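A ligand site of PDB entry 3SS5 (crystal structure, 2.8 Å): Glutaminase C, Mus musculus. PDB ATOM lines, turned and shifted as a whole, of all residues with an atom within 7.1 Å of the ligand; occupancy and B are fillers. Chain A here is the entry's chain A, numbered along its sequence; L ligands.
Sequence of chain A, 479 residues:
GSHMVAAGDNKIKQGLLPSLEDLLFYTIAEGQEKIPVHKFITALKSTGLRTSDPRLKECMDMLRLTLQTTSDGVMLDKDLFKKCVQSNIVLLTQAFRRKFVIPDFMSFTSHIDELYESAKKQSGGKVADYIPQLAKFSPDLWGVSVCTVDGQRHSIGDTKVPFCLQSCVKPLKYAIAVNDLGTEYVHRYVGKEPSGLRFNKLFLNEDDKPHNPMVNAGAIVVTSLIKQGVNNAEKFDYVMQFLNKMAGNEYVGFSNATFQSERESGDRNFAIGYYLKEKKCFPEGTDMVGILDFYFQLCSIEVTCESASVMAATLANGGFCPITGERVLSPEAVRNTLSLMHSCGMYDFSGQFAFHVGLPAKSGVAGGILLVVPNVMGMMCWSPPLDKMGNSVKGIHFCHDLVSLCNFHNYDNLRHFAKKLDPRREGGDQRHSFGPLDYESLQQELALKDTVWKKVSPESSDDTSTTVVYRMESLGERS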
ATOM      1  N   TYR A 130     -11.639  -5.457  17.925  1.00  0.00           N
ATOM      2  CA  TYR A 130     -10.245  -5.796  18.232  1.00  0.00           C
ATOM      3  C   TYR A 130      -9.282  -4.625  18.072  1.00  0.00           C
ATOM      4  O   TYR A 130      -8.175  -4.629  18.604  1.00  0.00           O
ATOM      5  CB  TYR A 130      -9.771  -7.038  17.458  1.00  0.00           C
ATOM      6  CG  TYR A 130      -9.320  -6.774  16.043  1.00  0.00           C
ATOM      7  CD1 TYR A 130      -8.012  -6.371  15.783  1.00  0.00           C
ATOM      8  CD2 TYR A 130     -10.178  -6.951  14.977  1.00  0.00           C
ATOM      9  CE1 TYR A 130      -7.595  -6.140  14.482  1.00  0.00           C
ATOM     10  CE2 TYR A 130      -9.767  -6.728  13.674  1.00  0.00           C
ATOM     11  CZ  TYR A 130      -8.468  -6.325  13.440  1.00  0.00           C
ATOM     12  OH  TYR A 130      -8.053  -6.082  12.147  1.00  0.00           O
ATOM     13  N   LEU A 134     -12.125  -0.089  13.992  1.00  0.00           N
ATOM     14  CA  LEU A 134     -13.247  -0.897  13.548  1.00  0.00           C
ATOM     15  C   LEU A 134     -14.457  -0.720  14.460  1.00  0.00           C
ATOM     16  O   LEU A 134     -15.594  -0.713  13.999  1.00  0.00           O
ATOM     17  CB  LEU A 134     -12.859  -2.380  13.485  1.00  0.00           C
ATOM     18  CG  LEU A 134     -11.793  -2.747  12.449  1.00  0.00           C
ATOM     19  CD1 LEU A 134     -11.351  -4.178  12.646  1.00  0.00           C
ATOM     20  CD2 LEU A 134     -12.323  -2.531  11.038  1.00  0.00           C
ATOM     21  N   LEU A 165      -9.954  -2.261   3.437  1.00  0.00           N
ATOM     22  CA  LEU A 165     -10.217  -3.509   2.744  1.00  0.00           C
ATOM     23  C   LEU A 165      -9.993  -4.706   3.659  1.00  0.00           C
ATOM     24  O   LEU A 165     -10.769  -5.660   3.644  1.00  0.00           O
ATOM     25  CB  LEU A 165      -9.327  -3.641   1.506  1.00  0.00           C
ATOM     26  CG  LEU A 165      -9.716  -2.797   0.291  1.00  0.00           C
ATOM     27  CD1 LEU A 165      -8.618  -2.829  -0.753  1.00  0.00           C
ATOM     28  CD2 LEU A 165     -11.038  -3.281  -0.288  1.00  0.00           C
ATOM     29  N   GLN A 166      -8.944  -4.648   4.473  1.00  0.00           N
ATOM     30  CA  GLN A 166      -8.568  -5.762   5.331  1.00  0.00           C
ATOM     31  C   GLN A 166      -8.289  -7.006   4.482  1.00  0.00           C
ATOM     32  O   GLN A 166      -7.439  -6.968   3.602  1.00  0.00           O
ATOM     33  CB  GLN A 166      -9.655  -6.040   6.368  1.00  0.00           C
ATOM     34  CG  GLN A 166      -9.801  -4.937   7.416  1.00  0.00           C
ATOM     35  CD  GLN A 166      -8.595  -4.831   8.331  1.00  0.00           C
ATOM     36  OE1 GLN A 166      -7.715  -5.700   8.331  1.00  0.00           O
ATOM     37  NE2 GLN A 166      -8.541  -3.759   9.111  1.00  0.00           N
ATOM     38  N   SER A 167      -9.019  -8.084   4.741  1.00  0.00           N
ATOM     39  CA  SER A 167      -8.830  -9.312   3.980  1.00  0.00           C
ATOM     40  C   SER A 167      -9.341  -9.206   2.550  1.00  0.00           C
ATOM     41  O   SER A 167      -9.027 -10.059   1.710  1.00  0.00           O
ATOM     42  CB  SER A 167      -9.482 -10.498   4.690  1.00  0.00           C
ATOM     43  OG  SER A 167      -8.668 -10.982   5.735  1.00  0.00           O
ATOM     44  N   CYS A 168     -10.124  -8.173   2.259  1.00  0.00           N
ATOM     45  CA  CYS A 168     -10.605  -7.933   0.903  1.00  0.00           C
ATOM     46  C   CYS A 168      -9.449  -7.652  -0.051  1.00  0.00           C
ATOM     47  O   CYS A 168      -9.591  -7.773  -1.271  1.00  0.00           O
ATOM     48  CB  CYS A 168     -11.600  -6.780   0.872  1.00  0.00           C
ATOM     49  SG  CYS A 168     -13.105  -7.029   1.848  1.00  0.00           S
ATOM     50  N   LYS A 170      -6.654  -9.317  -0.013  1.00  0.00           N
ATOM     51  CA  LYS A 170      -5.971 -10.588  -0.281  1.00  0.00           C
ATOM     52  C   LYS A 170      -6.027 -11.033  -1.745  1.00  0.00           C
ATOM     53  O   LYS A 170      -4.998 -11.320  -2.341  1.00  0.00           O
ATOM     54  CB  LYS A 170      -6.471 -11.696   0.655  1.00  0.00           C
ATOM     55  CG  LYS A 170      -6.014 -11.534   2.084  1.00  0.00           C
ATOM     56  CD  LYS A 170      -6.472 -12.669   2.967  1.00  0.00           C
ATOM     57  CE  LYS A 170      -5.871 -12.564   4.361  1.00  0.00           C
ATOM     58  NZ  LYS A 170      -6.200 -11.264   5.007  1.00  0.00           N
ATOM     59  N   ASN A 216      -4.478 -15.723   6.104  1.00  0.00           N
ATOM     60  CA  ASN A 216      -3.396 -14.848   6.551  1.00  0.00           C
ATOM     61  C   ASN A 216      -2.003 -15.394   6.245  1.00  0.00           C
ATOM     62  O   ASN A 216      -1.162 -14.683   5.698  1.00  0.00           O
ATOM     63  CB  ASN A 216      -3.514 -14.555   8.055  1.00  0.00           C
ATOM     64  CG  ASN A 216      -4.716 -13.685   8.385  1.00  0.00           C
ATOM     65  OD1 ASN A 216      -5.667 -13.610   7.609  1.00  0.00           O
ATOM     66  ND2 ASN A 216      -4.670 -13.031   9.538  1.00  0.00           N
ATOM     67  N   ILE A 220       0.357 -13.548   3.708  1.00  0.00           N
ATOM     68  CA  ILE A 220       1.641 -13.024   4.154  1.00  0.00           C
ATOM     69  C   ILE A 220       2.770 -13.421   3.199  1.00  0.00           C
ATOM     70  O   ILE A 220       3.646 -12.612   2.885  1.00  0.00           O
ATOM     71  CB  ILE A 220       1.988 -13.479   5.584  1.00  0.00           C
ATOM     72  CG1 ILE A 220       1.034 -12.816   6.586  1.00  0.00           C
ATOM     73  CG2 ILE A 220       3.429 -13.139   5.922  1.00  0.00           C
ATOM     74  CD1 ILE A 220       1.275 -13.235   8.026  1.00  0.00           C
ATOM     75  N   GLU A 262      -3.168  -1.964  14.038  1.00  0.00           N
ATOM     76  CA  GLU A 262      -2.985  -3.295  13.474  1.00  0.00           C
ATOM     77  C   GLU A 262      -1.654  -3.896  13.923  1.00  0.00           C
ATOM     78  O   GLU A 262      -1.581  -5.075  14.270  1.00  0.00           O
ATOM     79  CB  GLU A 262      -3.055  -3.229  11.948  1.00  0.00           C
ATOM     80  CG  GLU A 262      -3.495  -4.521  11.282  1.00  0.00           C
ATOM     81  CD  GLU A 262      -4.971  -4.797  11.481  1.00  0.00           C
ATOM     82  OE1 GLU A 262      -5.378  -5.973  11.392  1.00  0.00           O
ATOM     83  OE2 GLU A 262      -5.736  -3.841  11.726  1.00  0.00           O
ATOM     84  N   ARG A 268      -1.049 -12.589  16.480  1.00  0.00           N
ATOM     85  CA  ARG A 268      -1.421 -13.733  15.655  1.00  0.00           C
ATOM     86  C   ARG A 268      -0.565 -13.834  14.399  1.00  0.00           C
ATOM     87  O   ARG A 268       0.036 -14.877  14.117  1.00  0.00           O
ATOM     88  CB  ARG A 268      -2.901 -13.660  15.258  1.00  0.00           C
ATOM     89  CG  ARG A 268      -3.248 -14.569  14.075  1.00  0.00           C
ATOM     90  CD  ARG A 268      -4.728 -14.552  13.743  1.00  0.00           C
ATOM     91  NE  ARG A 268      -4.985 -15.235  12.472  1.00  0.00           N
ATOM     92  CZ  ARG A 268      -4.844 -16.540  12.284  1.00  0.00           C
ATOM     93  NH1 ARG A 268      -4.444 -17.318  13.281  1.00  0.00           N
ATOM     94  NH2 ARG A 268      -5.097 -17.071  11.094  1.00  0.00           N
ATOM     95  N   ASN A 269      -0.511 -12.743  13.637  1.00  0.00           N
ATOM     96  CA  ASN A 269       0.226 -12.709  12.388  1.00  0.00           C
ATOM     97  C   ASN A 269       1.734 -12.795  12.578  1.00  0.00           C
ATOM     98  O   ASN A 269       2.452 -13.288  11.718  1.00  0.00           O
ATOM     99  CB  ASN A 269      -0.139 -11.455  11.591  1.00  0.00           C
ATOM    100  CG  ASN A 269      -1.568 -11.497  11.065  1.00  0.00           C
ATOM    101  OD1 ASN A 269      -1.998 -12.503  10.480  1.00  0.00           O
ATOM    102  ND2 ASN A 269      -2.317 -10.429  11.282  1.00  0.00           N
ATOM    103  N   TYR A 295       2.345  -6.063   5.056  1.00  0.00           N
ATOM    104  CA  TYR A 295       1.073  -6.773   5.184  1.00  0.00           C
ATOM    105  C   TYR A 295       0.021  -5.918   5.896  1.00  0.00           C
ATOM    106  O   TYR A 295      -1.103  -5.788   5.414  1.00  0.00           O
ATOM    107  CB  TYR A 295       1.265  -8.088   5.927  1.00  0.00           C
ATOM    108  CG  TYR A 295      -0.028  -8.817   6.220  1.00  0.00           C
ATOM    109  CD1 TYR A 295      -0.539  -9.771   5.346  1.00  0.00           C
ATOM    110  CD2 TYR A 295      -0.755  -8.553   7.376  1.00  0.00           C
ATOM    111  CE1 TYR A 295      -1.724 -10.428   5.603  1.00  0.00           C
ATOM    112  CE2 TYR A 295      -1.940  -9.202   7.649  1.00  0.00           C
ATOM    113  CZ  TYR A 295      -2.413 -10.140   6.759  1.00  0.00           C
ATOM    114  OH  TYR A 295      -3.597 -10.790   7.032  1.00  0.00           O
ATOM    115  N   PHE A 296       0.382  -5.351   7.042  1.00  0.00           N
ATOM    116  CA  PHE A 296      -0.548  -4.539   7.817  1.00  0.00           C
ATOM    117  C   PHE A 296      -0.993  -3.300   7.052  1.00  0.00           C
ATOM    118  O   PHE A 296      -2.145  -2.865   7.176  1.00  0.00           O
ATOM    119  CB  PHE A 296       0.070  -4.154   9.166  1.00  0.00           C
ATOM    120  CG  PHE A 296       0.257  -5.307  10.107  1.00  0.00           C
ATOM    121  CD1 PHE A 296       1.427  -5.441  10.845  1.00  0.00           C
ATOM    122  CD2 PHE A 296      -0.732  -6.257  10.266  1.00  0.00           C
ATOM    123  CE1 PHE A 296       1.596  -6.507  11.707  1.00  0.00           C
ATOM    124  CE2 PHE A 296      -0.570  -7.319  11.134  1.00  0.00           C
ATOM    125  CZ  PHE A 296       0.594  -7.444  11.854  1.00  0.00           C
ATOM    126  N   CYS A 299      -3.612  -4.196   4.410  1.00  0.00           N
ATOM    127  CA  CYS A 299      -4.904  -4.369   5.065  1.00  0.00           C
ATOM    128  C   CYS A 299      -5.504  -3.023   5.440  1.00  0.00           C
ATOM    129  O   CYS A 299      -6.724  -2.880   5.561  1.00  0.00           O
ATOM    130  CB  CYS A 299      -4.779  -5.234   6.315  1.00  0.00           C
ATOM    131  SG  CYS A 299      -4.250  -6.932   6.024  1.00  0.00           S
ATOM    132  N   SER A 300      -4.634  -2.036   5.630  1.00  0.00           N
ATOM    133  CA  SER A 300      -5.056  -0.712   6.073  1.00  0.00           C
ATOM    134  C   SER A 300      -5.477   0.188   4.923  1.00  0.00           C
ATOM    135  O   SER A 300      -6.009   1.277   5.134  1.00  0.00           O
ATOM    136  CB  SER A 300      -3.937  -0.054   6.878  1.00  0.00           C
ATOM    137  OG  SER A 300      -3.465  -0.925   7.882  1.00  0.00           O
ATOM    138  N   TYR A 347     -14.041 -17.113   4.366  1.00  0.00           N
ATOM    139  CA  TYR A 347     -13.591 -17.713   5.633  1.00  0.00           C
ATOM    140  C   TYR A 347     -14.066 -19.146   5.774  1.00  0.00           C
ATOM    141  O   TYR A 347     -13.837 -19.973   4.883  1.00  0.00           O
ATOM    142  CB  TYR A 347     -14.062 -16.904   6.851  1.00  0.00           C
ATOM    143  CG  TYR A 347     -13.537 -15.499   6.950  1.00  0.00           C
ATOM    144  CD1 TYR A 347     -12.177 -15.258   7.084  1.00  0.00           C
ATOM    145  CD2 TYR A 347     -14.395 -14.409   6.921  1.00  0.00           C
ATOM    146  CE1 TYR A 347     -11.694 -13.975   7.181  1.00  0.00           C
ATOM    147  CE2 TYR A 347     -13.921 -13.129   7.006  1.00  0.00           C
ATOM    148  CZ  TYR A 347     -12.575 -12.916   7.142  1.00  0.00           C
ATOM    149  OH  TYR A 347     -12.108 -11.632   7.233  1.00  0.00           O
ATOM    150  N   LYS A 362     -14.924 -11.969  -1.696  1.00  0.00           N
ATOM    151  CA  LYS A 362     -14.000 -11.830  -0.578  1.00  0.00           C
ATOM    152  C   LYS A 362     -14.611 -10.969   0.504  1.00  0.00           C
ATOM    153  O   LYS A 362     -15.264  -9.969   0.220  1.00  0.00           O
ATOM    154  CB  LYS A 362     -12.665 -11.239  -1.032  1.00  0.00           C
ATOM    155  CG  LYS A 362     -11.580 -11.340   0.029  1.00  0.00           C
ATOM    156  CD  LYS A 362     -11.190 -12.787   0.282  1.00  0.00           C
ATOM    157  CE  LYS A 362     -10.496 -12.948   1.617  1.00  0.00           C
ATOM    158  NZ  LYS A 362     -11.431 -12.782   2.759  1.00  0.00           N
ATOM    159  N   SER A 363     -14.401 -11.363   1.754  1.00  0.00           N
ATOM    160  CA  SER A 363     -14.941 -10.634   2.893  1.00  0.00           C
ATOM    161  C   SER A 363     -13.802 -10.153   3.775  1.00  0.00           C
ATOM    162  O   SER A 363     -12.679 -10.642   3.691  1.00  0.00           O
ATOM    163  CB  SER A 363     -15.891 -11.516   3.696  1.00  0.00           C
ATOM    164  OG  SER A 363     -15.253 -12.690   4.141  1.00  0.00           O
ATOM    165  N   GLY A 364     -14.103  -9.174   4.630  1.00  0.00           N
ATOM    166  CA  GLY A 364     -13.096  -8.606   5.499  1.00  0.00           C
ATOM    167  C   GLY A 364     -13.700  -8.185   6.815  1.00  0.00           C
ATOM    168  O   GLY A 364     -14.924  -8.079   6.942  1.00  0.00           O
ATOM    169  N   VAL A 365     -12.850  -7.956   7.806  1.00  0.00           N
ATOM    170  CA  VAL A 365     -13.301  -7.681   9.156  1.00  0.00           C
ATOM    171  C   VAL A 365     -14.024  -6.343   9.248  1.00  0.00           C
ATOM    172  O   VAL A 365     -14.803  -6.099  10.161  1.00  0.00           O
ATOM    173  CB  VAL A 365     -12.125  -7.729  10.153  1.00  0.00           C
ATOM    174  CG1 VAL A 365     -11.322  -6.453  10.083  1.00  0.00           C
ATOM    175  CG2 VAL A 365     -12.643  -7.970  11.568  1.00  0.00           C
ATOM    176  N   ALA A 366     -13.763  -5.471   8.281  1.00  0.00           N
ATOM    177  CA  ALA A 366     -14.410  -4.163   8.234  1.00  0.00           C
ATOM    178  C   ALA A 366     -15.888  -4.304   7.875  1.00  0.00           C
ATOM    179  O   ALA A 366     -16.673  -3.377   8.052  1.00  0.00           O
ATOM    180  CB  ALA A 366     -13.708  -3.260   7.233  1.00  0.00           C
ATOM    181  N   GLY A 390     -17.561 -14.292  10.732  1.00  0.00           N
ATOM    182  CA  GLY A 390     -16.730 -13.131  10.458  1.00  0.00           C
ATOM    183  C   GLY A 390     -17.153 -12.415   9.197  1.00  0.00           C
ATOM    184  O   GLY A 390     -16.484 -11.477   8.740  1.00  0.00           O
HETATM  185  N1  LIG L   1      -5.643  -7.407   9.165  1.00  0.00           N
HETATM  186  C1  LIG L   1      -6.467  -8.425   9.813  1.00  0.00           C
HETATM  187  C2  LIG L   1      -5.633  -9.651  10.159  1.00  0.00           C
HETATM  188  O1  LIG L   1      -5.961 -10.389  11.093  1.00  0.00           O
HETATM  189  C3  LIG L   1      -7.633  -8.820   8.917  1.00  0.00           C
HETATM  190  C4  LIG L   1      -8.502  -9.923   9.487  1.00  0.00           C
HETATM  191  C5  LIG L   1      -9.587 -10.358   8.528  1.00  0.00           C
HETATM  192  O2  LIG L   1      -9.906 -11.564   8.499  1.00  0.00           O
HETATM  193  O3  LIG L   1     -10.135  -9.489   7.813  1.00  0.00           O
HETATM  194  O4  LIG L   1      -4.626  -9.948   9.518  1.00  0.00           O
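The side-chain hydroxyl (OH) of Tyr 347 sits at hydrogen-bond distance from an oxygen (O2) of the ligand.
N1 of the ligand lies within salt-bridge range of OE1 of Glu 262 (2.7 Å).
The side-chain amide oxygen (OE1) of Gln 166 sits at hydrogen-bond distance from a nitrogen (N1) of the ligand, at 2.8 Å.
An oxygen (O4) of the ligand sits at hydrogen-bond distance from the side-chain hydroxyl (OH) of Tyr 295 (2.8 Å).
O4 of the ligand lies within hydrogen-bond range of ND2 of Asn 269 (2.9 Å).
The side-chain hydroxyl (OG) of Ser 167 is in hydrogen-bond range of an oxygen (O3) of the ligand, at 2.9 Å.
O4 of the ligand is in hydrogen-bond range of ND2 of Asn 216, 3.1 Å away.
N of Val 365 is in hydrogen-bond range of O3 of the ligand (3.1 Å).
The side-chain sulfur (SG) of Cys 299 lies within hydrogen-bond range of a nitrogen (N1) of the ligand.
The side-chain hydroxyl (OH) of Tyr 130 lies within hydrogen-bond range of the side-chain carboxylate (OE1) of Glu 262, at 2.8 Å.
O of Cys 299 is in hydrogen-bond range of N of Gln 166.
The backbone carbonyl oxygen (O) of Tyr 295 lies within hydrogen-bond range of the side-chain sulfur (SG) of Cys 299, at 3.4 Å.
The side-chain hydroxyl (OH) of Tyr 295 lies within hydrogen-bond range of the side-chain amino group (NZ) of Lys 170 (3.3 Å).
The side-chain amide nitrogen (ND2) of Asn 216 is in hydrogen-bond range of the side-chain amide oxygen (OD1) of Asn 269, 2.9 Å away.
The side-chain amino group of Lys 170 sits at hydrogen-bond distance from the side-chain hydroxyl of Ser 167, 2.6 Å away.
The side-chain sulfur (SG) of Cys 168 sits at hydrogen-bond distance from the backbone NH (N) of Gly 364 (3.7 Å).
Residues that only touch the ligand: Tyr 130 (3.7 Å) and Gly 364 (3.9 Å).
Hydrophobic or aromatic side chains within 4 Å of the ligand: Tyr 295, Tyr 347 and Val 365.
11 residues have an atom within 4 Å of the ligand: Tyr 130, Gln 166, Ser 167, Asn 216, Glu 262, Asn 269, Tyr 295, Cys 299, Tyr 347, Gly 364 and Val 365.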
